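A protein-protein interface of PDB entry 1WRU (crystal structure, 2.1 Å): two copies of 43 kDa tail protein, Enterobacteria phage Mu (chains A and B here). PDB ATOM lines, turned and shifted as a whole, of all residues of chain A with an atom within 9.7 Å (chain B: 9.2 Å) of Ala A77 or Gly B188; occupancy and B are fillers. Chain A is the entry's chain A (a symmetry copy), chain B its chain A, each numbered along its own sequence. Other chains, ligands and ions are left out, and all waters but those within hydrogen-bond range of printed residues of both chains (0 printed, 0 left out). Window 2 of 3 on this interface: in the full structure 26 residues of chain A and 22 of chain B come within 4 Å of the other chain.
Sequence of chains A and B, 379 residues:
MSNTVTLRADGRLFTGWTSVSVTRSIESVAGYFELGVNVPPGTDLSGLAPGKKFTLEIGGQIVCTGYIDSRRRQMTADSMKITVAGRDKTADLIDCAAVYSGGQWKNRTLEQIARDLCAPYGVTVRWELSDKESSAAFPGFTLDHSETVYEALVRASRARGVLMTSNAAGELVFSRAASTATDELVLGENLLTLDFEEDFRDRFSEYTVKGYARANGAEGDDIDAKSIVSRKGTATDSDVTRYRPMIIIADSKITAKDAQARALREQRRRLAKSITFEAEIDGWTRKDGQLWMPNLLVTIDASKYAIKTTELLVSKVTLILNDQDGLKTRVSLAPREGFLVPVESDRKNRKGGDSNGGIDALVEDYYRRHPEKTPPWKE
No position is printed for both chains.
Of the 17 pairs that touch across the chains among the printed residues, none has its exchanged pair printed and touching as well.
O of Leu B194 touches CA of Gln A74, at 3.4 Å.
Thr B193 touches Met A75.
SD of Met A75 touches CD1 of Tyr B305, 3.8 Å away.
Thr A76 touches Leu B192 (CA to O, 3.7 Å).
Thr A76 touches Thr B193.
Gly B188 touches Ala A77.
CE of Lys B304 touches O of Ala A77, 2.8 Å away.
Tyr B305 touches Ala A77.
CE of Lys B304 touches O of Asp A78, 3.99 Å away.
Met A80 touches Tyr B305.
OH of Tyr B305 sits at hydrogen-bond distance from O of Asp A78, 2.9 Å away.
OH of Tyr B305 lies close to N of Ser A79 (3.1 Å).
The backbone NH (N) of Met A75 lies within hydrogen-bond range of the backbone carbonyl oxygen (O) of Leu B194 (2.7 Å).
Of the 10 printed residues of chain A, 8 touch a printed residue of chain B.
Hydrophobic or aromatic side chains of chain A that line the printed part of chain B: Pro A41, Met A75, Ala A77 and Met A80.
Of the 18 printed residues of chain B, 7 touch a printed residue of chain A.
Among the printed residues, no Asp or Glu carboxylate lies within 4 Å of a Lys or Arg side-chain nitrogen of the other chain.
Printed residues of chain B within 4 Å of Met A75: Thr B193, Leu B194 and Tyr B305.
Thr A76 touches four residues of chain B.
Ala A77 touches just these residues of chain B: Gly B188, Lys B304 and Tyr B305.
Printed residues of chain A within 4 Å of Leu B187: Thr A76.
Gly B188 touches one residue of chain A.
Of the printed residues of chain A, Leu B192 touches Thr A76 (3.7 Å).
The nearest printed residue of chain B that does not touch Ala A77 is Leu B187 (4.1 Å).
The nearest residue of chain A that does not touch Gly B188 is Thr A76 (5.9 Å).
The backbone NH of Ser A79 sits at hydrogen-bond distance from the side-chain hydroxyl of Thr A76, at 3.1 Å.
The backbone NH (N) of Asp A78 sits close to the side-chain hydroxyl (OG1) of Thr A76, at 3.2 Å.
The backbone NH (N) of Glu B280 sits at hydrogen-bond distance from the backbone carbonyl oxygen (O) of Thr B193 (2.8 Å).
O of Met A80 lies within hydrogen-bond range of N of Val A39 (3.0 Å).
The backbone NH (N) of Leu B192 sits at hydrogen-bond distance from the backbone carbonyl oxygen (O) of Glu B280 (2.8 Å).
The backbone NH of Leu B187 lies within hydrogen-bond range of the backbone carbonyl oxygen of Asp B301, at 3.0 Å.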
ATOM      1  N   VAL A  39      14.909 -17.721  23.069  1.00  0.00           N
ATOM      2  CA  VAL A  39      14.643 -16.557  22.235  1.00  0.00           C
ATOM      3  C   VAL A  39      14.890 -16.821  20.760  1.00  0.00           C
ATOM      4  O   VAL A  39      15.859 -17.478  20.387  1.00  0.00           O
ATOM      5  CB  VAL A  39      15.523 -15.363  22.641  1.00  0.00           C
ATOM      6  CG1 VAL A  39      15.165 -14.906  24.045  1.00  0.00           C
ATOM      7  CG2 VAL A  39      16.978 -15.753  22.568  1.00  0.00           C
ATOM      8  N   PRO A  40      14.002 -16.311  19.897  1.00  0.00           N
ATOM      9  CA  PRO A  40      14.155 -16.505  18.456  1.00  0.00           C
ATOM     10  C   PRO A  40      15.320 -15.665  17.957  1.00  0.00           C
ATOM     11  O   PRO A  40      15.542 -14.552  18.437  1.00  0.00           O
ATOM     12  CB  PRO A  40      12.821 -16.018  17.902  1.00  0.00           C
ATOM     13  CG  PRO A  40      11.871 -16.271  19.036  1.00  0.00           C
ATOM     14  CD  PRO A  40      12.666 -15.786  20.209  1.00  0.00           C
ATOM     15  N   PRO A  41      16.087 -16.193  16.991  1.00  0.00           N
ATOM     16  CA  PRO A  41      17.233 -15.466  16.440  1.00  0.00           C
ATOM     17  C   PRO A  41      16.883 -14.018  16.106  1.00  0.00           C
ATOM     18  O   PRO A  41      15.794 -13.732  15.614  1.00  0.00           O
ATOM     19  CB  PRO A  41      17.586 -16.283  15.203  1.00  0.00           C
ATOM     20  CG  PRO A  41      17.278 -17.683  15.649  1.00  0.00           C
ATOM     21  CD  PRO A  41      15.945 -17.514  16.350  1.00  0.00           C
ATOM     22  N   GLN A  74      23.086 -19.956  25.654  1.00  0.00           N
ATOM     23  CA  GLN A  74      23.455 -21.290  25.211  1.00  0.00           C
ATOM     24  C   GLN A  74      22.799 -21.470  23.847  1.00  0.00           C
ATOM     25  O   GLN A  74      21.568 -21.425  23.725  1.00  0.00           O
ATOM     26  CB  GLN A  74      22.947 -22.325  26.202  1.00  0.00           C
ATOM     27  CG  GLN A  74      23.645 -22.278  27.550  1.00  0.00           C
ATOM     28  CD  GLN A  74      22.819 -22.950  28.615  1.00  0.00           C
ATOM     29  OE1 GLN A  74      21.880 -22.359  29.147  1.00  0.00           O
ATOM     30  NE2 GLN A  74      23.137 -24.200  28.906  1.00  0.00           N
ATOM     31  N   MET A  75      23.608 -21.676  22.816  1.00  0.00           N
ATOM     32  CA  MET A  75      23.046 -21.810  21.484  1.00  0.00           C
ATOM     33  C   MET A  75      23.489 -22.977  20.619  1.00  0.00           C
ATOM     34  O   MET A  75      24.550 -23.561  20.816  1.00  0.00           O
ATOM     35  CB  MET A  75      23.272 -20.507  20.722  1.00  0.00           C
ATOM     36  CG  MET A  75      24.709 -20.084  20.629  1.00  0.00           C
ATOM     37  SD  MET A  75      24.872 -18.290  20.718  1.00  0.00           S
ATOM     38  CE  MET A  75      25.758 -18.118  22.297  1.00  0.00           C
ATOM     39  N   THR A  76      22.623 -23.321  19.673  1.00  0.00           N
ATOM     40  CA  THR A  76      22.875 -24.373  18.699  1.00  0.00           C
ATOM     41  C   THR A  76      22.549 -23.680  17.398  1.00  0.00           C
ATOM     42  O   THR A  76      22.151 -22.511  17.402  1.00  0.00           O
ATOM     43  CB  THR A  76      21.916 -25.560  18.840  1.00  0.00           C
ATOM     44  OG1 THR A  76      20.565 -25.097  18.739  1.00  0.00           O
ATOM     45  CG2 THR A  76      22.124 -26.264  20.167  1.00  0.00           C
ATOM     46  N   ALA A  77      22.714 -24.384  16.285  1.00  0.00           N
ATOM     47  CA  ALA A  77      22.410 -23.794  14.993  1.00  0.00           C
ATOM     48  C   ALA A  77      20.940 -23.380  14.984  1.00  0.00           C
ATOM     49  O   ALA A  77      20.577 -22.369  14.396  1.00  0.00           O
ATOM     50  CB  ALA A  77      22.687 -24.800  13.882  1.00  0.00           C
ATOM     51  N   ASP A  78      20.112 -24.163  15.669  1.00  0.00           N
ATOM     52  CA  ASP A  78      18.670 -23.931  15.752  1.00  0.00           C
ATOM     53  C   ASP A  78      18.168 -22.862  16.717  1.00  0.00           C
ATOM     54  O   ASP A  78      17.492 -21.923  16.299  1.00  0.00           O
ATOM     55  CB  ASP A  78      17.947 -25.238  16.087  1.00  0.00           C
ATOM     56  CG  ASP A  78      17.688 -26.096  14.865  1.00  0.00           C
ATOM     57  OD1 ASP A  78      17.173 -27.223  15.031  1.00  0.00           O
ATOM     58  OD2 ASP A  78      17.992 -25.642  13.741  1.00  0.00           O
ATOM     59  N   SER A  79      18.470 -23.002  18.005  1.00  0.00           N
ATOM     60  CA  SER A  79      17.972 -22.031  18.981  1.00  0.00           C
ATOM     61  C   SER A  79      18.933 -21.621  20.087  1.00  0.00           C
ATOM     62  O   SER A  79      20.020 -22.181  20.242  1.00  0.00           O
ATOM     63  CB  SER A  79      16.709 -22.567  19.630  1.00  0.00           C
ATOM     64  OG  SER A  79      17.017 -23.713  20.398  1.00  0.00           O
ATOM     65  N   MET A  80      18.492 -20.645  20.875  1.00  0.00           N
ATOM     66  CA  MET A  80      19.282 -20.132  21.979  1.00  0.00           C
ATOM     67  C   MET A  80      18.471 -19.966  23.250  1.00  0.00           C
ATOM     68  O   MET A  80      17.336 -19.487  23.215  1.00  0.00           O
ATOM     69  CB  MET A  80      19.890 -18.785  21.601  1.00  0.00           C
ATOM     70  CG  MET A  80      20.618 -18.093  22.738  1.00  0.00           C
ATOM     71  SD  MET A  80      21.368 -16.590  22.143  1.00  0.00           S
ATOM     72  CE  MET A  80      19.977 -15.531  22.102  1.00  0.00           C
ATOM     73  N   LEU B 185      35.766 -20.342  14.803  1.00  0.00           N
ATOM     74  CA  LEU B 185      34.660 -21.206  15.166  1.00  0.00           C
ATOM     75  C   LEU B 185      33.439 -20.533  14.592  1.00  0.00           C
ATOM     76  O   LEU B 185      33.186 -19.358  14.858  1.00  0.00           O
ATOM     77  CB  LEU B 185      34.533 -21.321  16.695  1.00  0.00           C
ATOM     78  CG  LEU B 185      35.791 -21.864  17.379  1.00  0.00           C
ATOM     79  CD1 LEU B 185      35.561 -22.099  18.880  1.00  0.00           C
ATOM     80  CD2 LEU B 185      36.174 -23.164  16.681  1.00  0.00           C
ATOM     81  N   VAL B 186      32.683 -21.283  13.802  1.00  0.00           N
ATOM     82  CA  VAL B 186      31.492 -20.748  13.176  1.00  0.00           C
ATOM     83  C   VAL B 186      30.292 -21.580  13.558  1.00  0.00           C
ATOM     84  O   VAL B 186      30.249 -22.791  13.303  1.00  0.00           O
ATOM     85  CB  VAL B 186      31.660 -20.725  11.631  1.00  0.00           C
ATOM     86  CG1 VAL B 186      30.396 -20.196  10.971  1.00  0.00           C
ATOM     87  CG2 VAL B 186      32.849 -19.870  11.281  1.00  0.00           C
ATOM     88  N   LEU B 187      29.318 -20.930  14.185  1.00  0.00           N
ATOM     89  CA  LEU B 187      28.131 -21.636  14.618  1.00  0.00           C
ATOM     90  C   LEU B 187      27.403 -22.289  13.440  1.00  0.00           C
ATOM     91  O   LEU B 187      27.155 -21.647  12.425  1.00  0.00           O
ATOM     92  CB  LEU B 187      27.198 -20.678  15.360  1.00  0.00           C
ATOM     93  CG  LEU B 187      25.926 -21.340  15.887  1.00  0.00           C
ATOM     94  CD1 LEU B 187      26.294 -22.501  16.809  1.00  0.00           C
ATOM     95  CD2 LEU B 187      25.085 -20.311  16.616  1.00  0.00           C
ATOM     96  N   GLY B 188      27.067 -23.566  13.586  1.00  0.00           N
ATOM     97  CA  GLY B 188      26.363 -24.274  12.536  1.00  0.00           C
ATOM     98  C   GLY B 188      27.287 -25.120  11.688  1.00  0.00           C
ATOM     99  O   GLY B 188      26.859 -26.093  11.069  1.00  0.00           O
ATOM    100  N   GLU B 189      28.563 -24.754  11.672  1.00  0.00           N
ATOM    101  CA  GLU B 189      29.555 -25.469  10.897  1.00  0.00           C
ATOM    102  C   GLU B 189      30.444 -26.349  11.761  1.00  0.00           C
ATOM    103  O   GLU B 189      30.074 -27.471  12.100  1.00  0.00           O
ATOM    104  CB  GLU B 189      30.386 -24.464  10.108  1.00  0.00           C
ATOM    105  CG  GLU B 189      29.614 -23.900   8.932  1.00  0.00           C
ATOM    106  CD  GLU B 189      30.256 -22.672   8.343  1.00  0.00           C
ATOM    107  OE1 GLU B 189      31.495 -22.550   8.427  1.00  0.00           O
ATOM    108  OE2 GLU B 189      29.522 -21.836   7.781  1.00  0.00           O
ATOM    109  N   ASN B 190      31.626 -25.855  12.104  1.00  0.00           N
ATOM    110  CA  ASN B 190      32.516 -26.628  12.949  1.00  0.00           C
ATOM    111  C   ASN B 190      32.080 -26.459  14.419  1.00  0.00           C
ATOM    112  O   ASN B 190      32.407 -27.282  15.273  1.00  0.00           O
ATOM    113  CB  ASN B 190      33.961 -26.172  12.741  1.00  0.00           C
ATOM    114  CG  ASN B 190      34.142 -24.682  12.961  1.00  0.00           C
ATOM    115  OD1 ASN B 190      33.176 -23.917  12.953  1.00  0.00           O
ATOM    116  ND2 ASN B 190      35.387 -24.260  13.151  1.00  0.00           N
ATOM    117  N   LEU B 191      31.324 -25.400  14.698  1.00  0.00           N
ATOM    118  CA  LEU B 191      30.843 -25.144  16.053  1.00  0.00           C
ATOM    119  C   LEU B 191      29.409 -25.631  16.196  1.00  0.00           C
ATOM    120  O   LEU B 191      28.480 -24.983  15.723  1.00  0.00           O
ATOM    121  CB  LEU B 191      30.904 -23.651  16.365  1.00  0.00           C
ATOM    122  CG  LEU B 191      30.312 -23.227  17.713  1.00  0.00           C
ATOM    123  CD1 LEU B 191      31.210 -23.681  18.863  1.00  0.00           C
ATOM    124  CD2 LEU B 191      30.174 -21.712  17.731  1.00  0.00           C
ATOM    125  N   LEU B 192      29.234 -26.775  16.849  1.00  0.00           N
ATOM    126  CA  LEU B 192      27.918 -27.355  17.061  1.00  0.00           C
ATOM    127  C   LEU B 192      27.083 -26.628  18.130  1.00  0.00           C
ATOM    128  O   LEU B 192      25.890 -26.378  17.937  1.00  0.00           O
ATOM    129  CB  LEU B 192      28.066 -28.827  17.448  1.00  0.00           C
ATOM    130  CG  LEU B 192      28.869 -29.716  16.499  1.00  0.00           C
ATOM    131  CD1 LEU B 192      28.837 -31.146  17.006  1.00  0.00           C
ATOM    132  CD2 LEU B 192      28.279 -29.637  15.091  1.00  0.00           C
ATOM    133  N   THR B 193      27.703 -26.326  19.272  1.00  0.00           N
ATOM    134  CA  THR B 193      27.011 -25.626  20.348  1.00  0.00           C
ATOM    135  C   THR B 193      27.971 -24.658  21.013  1.00  0.00           C
ATOM    136  O   THR B 193      29.173 -24.907  21.096  1.00  0.00           O
ATOM    137  CB  THR B 193      26.480 -26.584  21.429  1.00  0.00           C
ATOM    138  OG1 THR B 193      27.583 -27.213  22.094  1.00  0.00           O
ATOM    139  CG2 THR B 193      25.577 -27.653  20.806  1.00  0.00           C
ATOM    140  N   LEU B 194      27.424 -23.539  21.465  1.00  0.00           N
ATOM    141  CA  LEU B 194      28.200 -22.519  22.137  1.00  0.00           C
ATOM    142  C   LEU B 194      27.456 -22.085  23.397  1.00  0.00           C
ATOM    143  O   LEU B 194      26.237 -21.834  23.360  1.00  0.00           O
ATOM    144  CB  LEU B 194      28.405 -21.321  21.224  1.00  0.00           C
ATOM    145  CG  LEU B 194      29.371 -20.306  21.820  1.00  0.00           C
ATOM    146  CD1 LEU B 194      30.762 -20.925  21.876  1.00  0.00           C
ATOM    147  CD2 LEU B 194      29.377 -19.045  20.988  1.00  0.00           C
ATOM    148  N   GLU B 280      31.242 -26.672  21.732  1.00  0.00           N
ATOM    149  CA  GLU B 280      31.239 -28.056  21.282  1.00  0.00           C
ATOM    150  C   GLU B 280      31.595 -28.051  19.785  1.00  0.00           C
ATOM    151  O   GLU B 280      30.816 -27.595  18.953  1.00  0.00           O
ATOM    152  CB  GLU B 280      29.877 -28.703  21.481  1.00  0.00           C
ATOM    153  CG  GLU B 280      29.809 -30.111  20.922  1.00  0.00           C
ATOM    154  CD  GLU B 280      29.153 -31.086  21.879  1.00  0.00           C
ATOM    155  OE1 GLU B 280      29.074 -32.289  21.543  1.00  0.00           O
ATOM    156  OE2 GLU B 280      28.718 -30.649  22.967  1.00  0.00           O
ATOM    157  N   ASP B 282      32.844 -30.112  16.243  1.00  0.00           N
ATOM    158  CA  ASP B 282      32.608 -31.425  15.658  1.00  0.00           C
ATOM    159  C   ASP B 282      33.991 -32.020  15.359  1.00  0.00           C
ATOM    160  O   ASP B 282      34.860 -31.330  14.854  1.00  0.00           O
ATOM    161  CB  ASP B 282      31.766 -31.274  14.392  1.00  0.00           C
ATOM    162  CG  ASP B 282      31.103 -32.571  13.972  1.00  0.00           C
ATOM    163  OD1 ASP B 282      30.665 -33.351  14.851  1.00  0.00           O
ATOM    164  OD2 ASP B 282      31.002 -32.798  12.754  1.00  0.00           O
ATOM    165  N   ILE B 300      35.258 -16.361  17.268  1.00  0.00           N
ATOM    166  CA  ILE B 300      33.994 -17.065  17.254  1.00  0.00           C
ATOM    167  C   ILE B 300      33.011 -16.239  16.485  1.00  0.00           C
ATOM    168  O   ILE B 300      32.994 -15.019  16.611  1.00  0.00           O
ATOM    169  CB  ILE B 300      33.425 -17.227  18.680  1.00  0.00           C
ATOM    170  CG1 ILE B 300      34.269 -18.219  19.481  1.00  0.00           C
ATOM    171  CG2 ILE B 300      31.981 -17.659  18.600  1.00  0.00           C
ATOM    172  CD1 ILE B 300      33.819 -18.419  20.930  1.00  0.00           C
ATOM    173  N   ASP B 301      32.193 -16.911  15.688  1.00  0.00           N
ATOM    174  CA  ASP B 301      31.166 -16.227  14.924  1.00  0.00           C
ATOM    175  C   ASP B 301      29.798 -16.888  15.091  1.00  0.00           C
ATOM    176  O   ASP B 301      29.528 -17.961  14.543  1.00  0.00           O
ATOM    177  CB  ASP B 301      31.535 -16.165  13.446  1.00  0.00           C
ATOM    178  CG  ASP B 301      30.484 -15.446  12.627  1.00  0.00           C
ATOM    179  OD1 ASP B 301      29.827 -14.543  13.187  1.00  0.00           O
ATOM    180  OD2 ASP B 301      30.325 -15.774  11.428  1.00  0.00           O
ATOM    181  N   ALA B 302      28.946 -16.230  15.868  1.00  0.00           N
ATOM    182  CA  ALA B 302      27.596 -16.695  16.139  1.00  0.00           C
ATOM    183  C   ALA B 302      26.672 -15.541  15.779  1.00  0.00           C
ATOM    184  O   ALA B 302      25.736 -15.213  16.525  1.00  0.00           O
ATOM    185  CB  ALA B 302      27.445 -17.053  17.619  1.00  0.00           C
ATOM    186  N   SER B 303      26.968 -14.923  14.633  1.00  0.00           N
ATOM    187  CA  SER B 303      26.208 -13.793  14.098  1.00  0.00           C
ATOM    188  C   SER B 303      24.706 -14.009  14.153  1.00  0.00           C
ATOM    189  O   SER B 303      23.952 -13.078  14.417  1.00  0.00           O
ATOM    190  CB  SER B 303      26.620 -13.528  12.649  1.00  0.00           C
ATOM    191  OG  SER B 303      27.953 -13.062  12.595  1.00  0.00           O
ATOM    192  N   LYS B 304      24.282 -15.239  13.887  1.00  0.00           N
ATOM    193  CA  LYS B 304      22.868 -15.595  13.913  1.00  0.00           C
ATOM    194  C   LYS B 304      22.239 -15.135  15.232  1.00  0.00           C
ATOM    195  O   LYS B 304      21.031 -14.915  15.311  1.00  0.00           O
ATOM    196  CB  LYS B 304      22.722 -17.111  13.752  1.00  0.00           C
ATOM    197  CG  LYS B 304      21.307 -17.626  13.849  1.00  0.00           C
ATOM    198  CD  LYS B 304      21.285 -19.142  13.777  1.00  0.00           C
ATOM    199  CE  LYS B 304      19.885 -19.695  14.014  1.00  0.00           C
ATOM    200  NZ  LYS B 304      18.904 -19.281  12.971  1.00  0.00           N
ATOM    201  N   TYR B 305      23.069 -14.988  16.262  1.00  0.00           N
ATOM    202  CA  TYR B 305      22.604 -14.550  17.570  1.00  0.00           C
ATOM    203  C   TYR B 305      23.365 -13.315  18.014  1.00  0.00           C
ATOM    204  O   TYR B 305      23.609 -13.106  19.212  1.00  0.00           O
ATOM    205  CB  TYR B 305      22.771 -15.670  18.586  1.00  0.00           C
ATOM    206  CG  TYR B 305      21.892 -16.852  18.281  1.00  0.00           C
ATOM    207  CD1 TYR B 305      22.434 -18.049  17.813  1.00  0.00           C
ATOM    208  CD2 TYR B 305      20.507 -16.770  18.445  1.00  0.00           C
ATOM    209  CE1 TYR B 305      21.616 -19.139  17.518  1.00  0.00           C
ATOM    210  CE2 TYR B 305      19.679 -17.857  18.156  1.00  0.00           C
ATOM    211  CZ  TYR B 305      20.240 -19.034  17.696  1.00  0.00           C
ATOM    212  OH  TYR B 305      19.433 -20.117  17.444  1.00  0.00           O
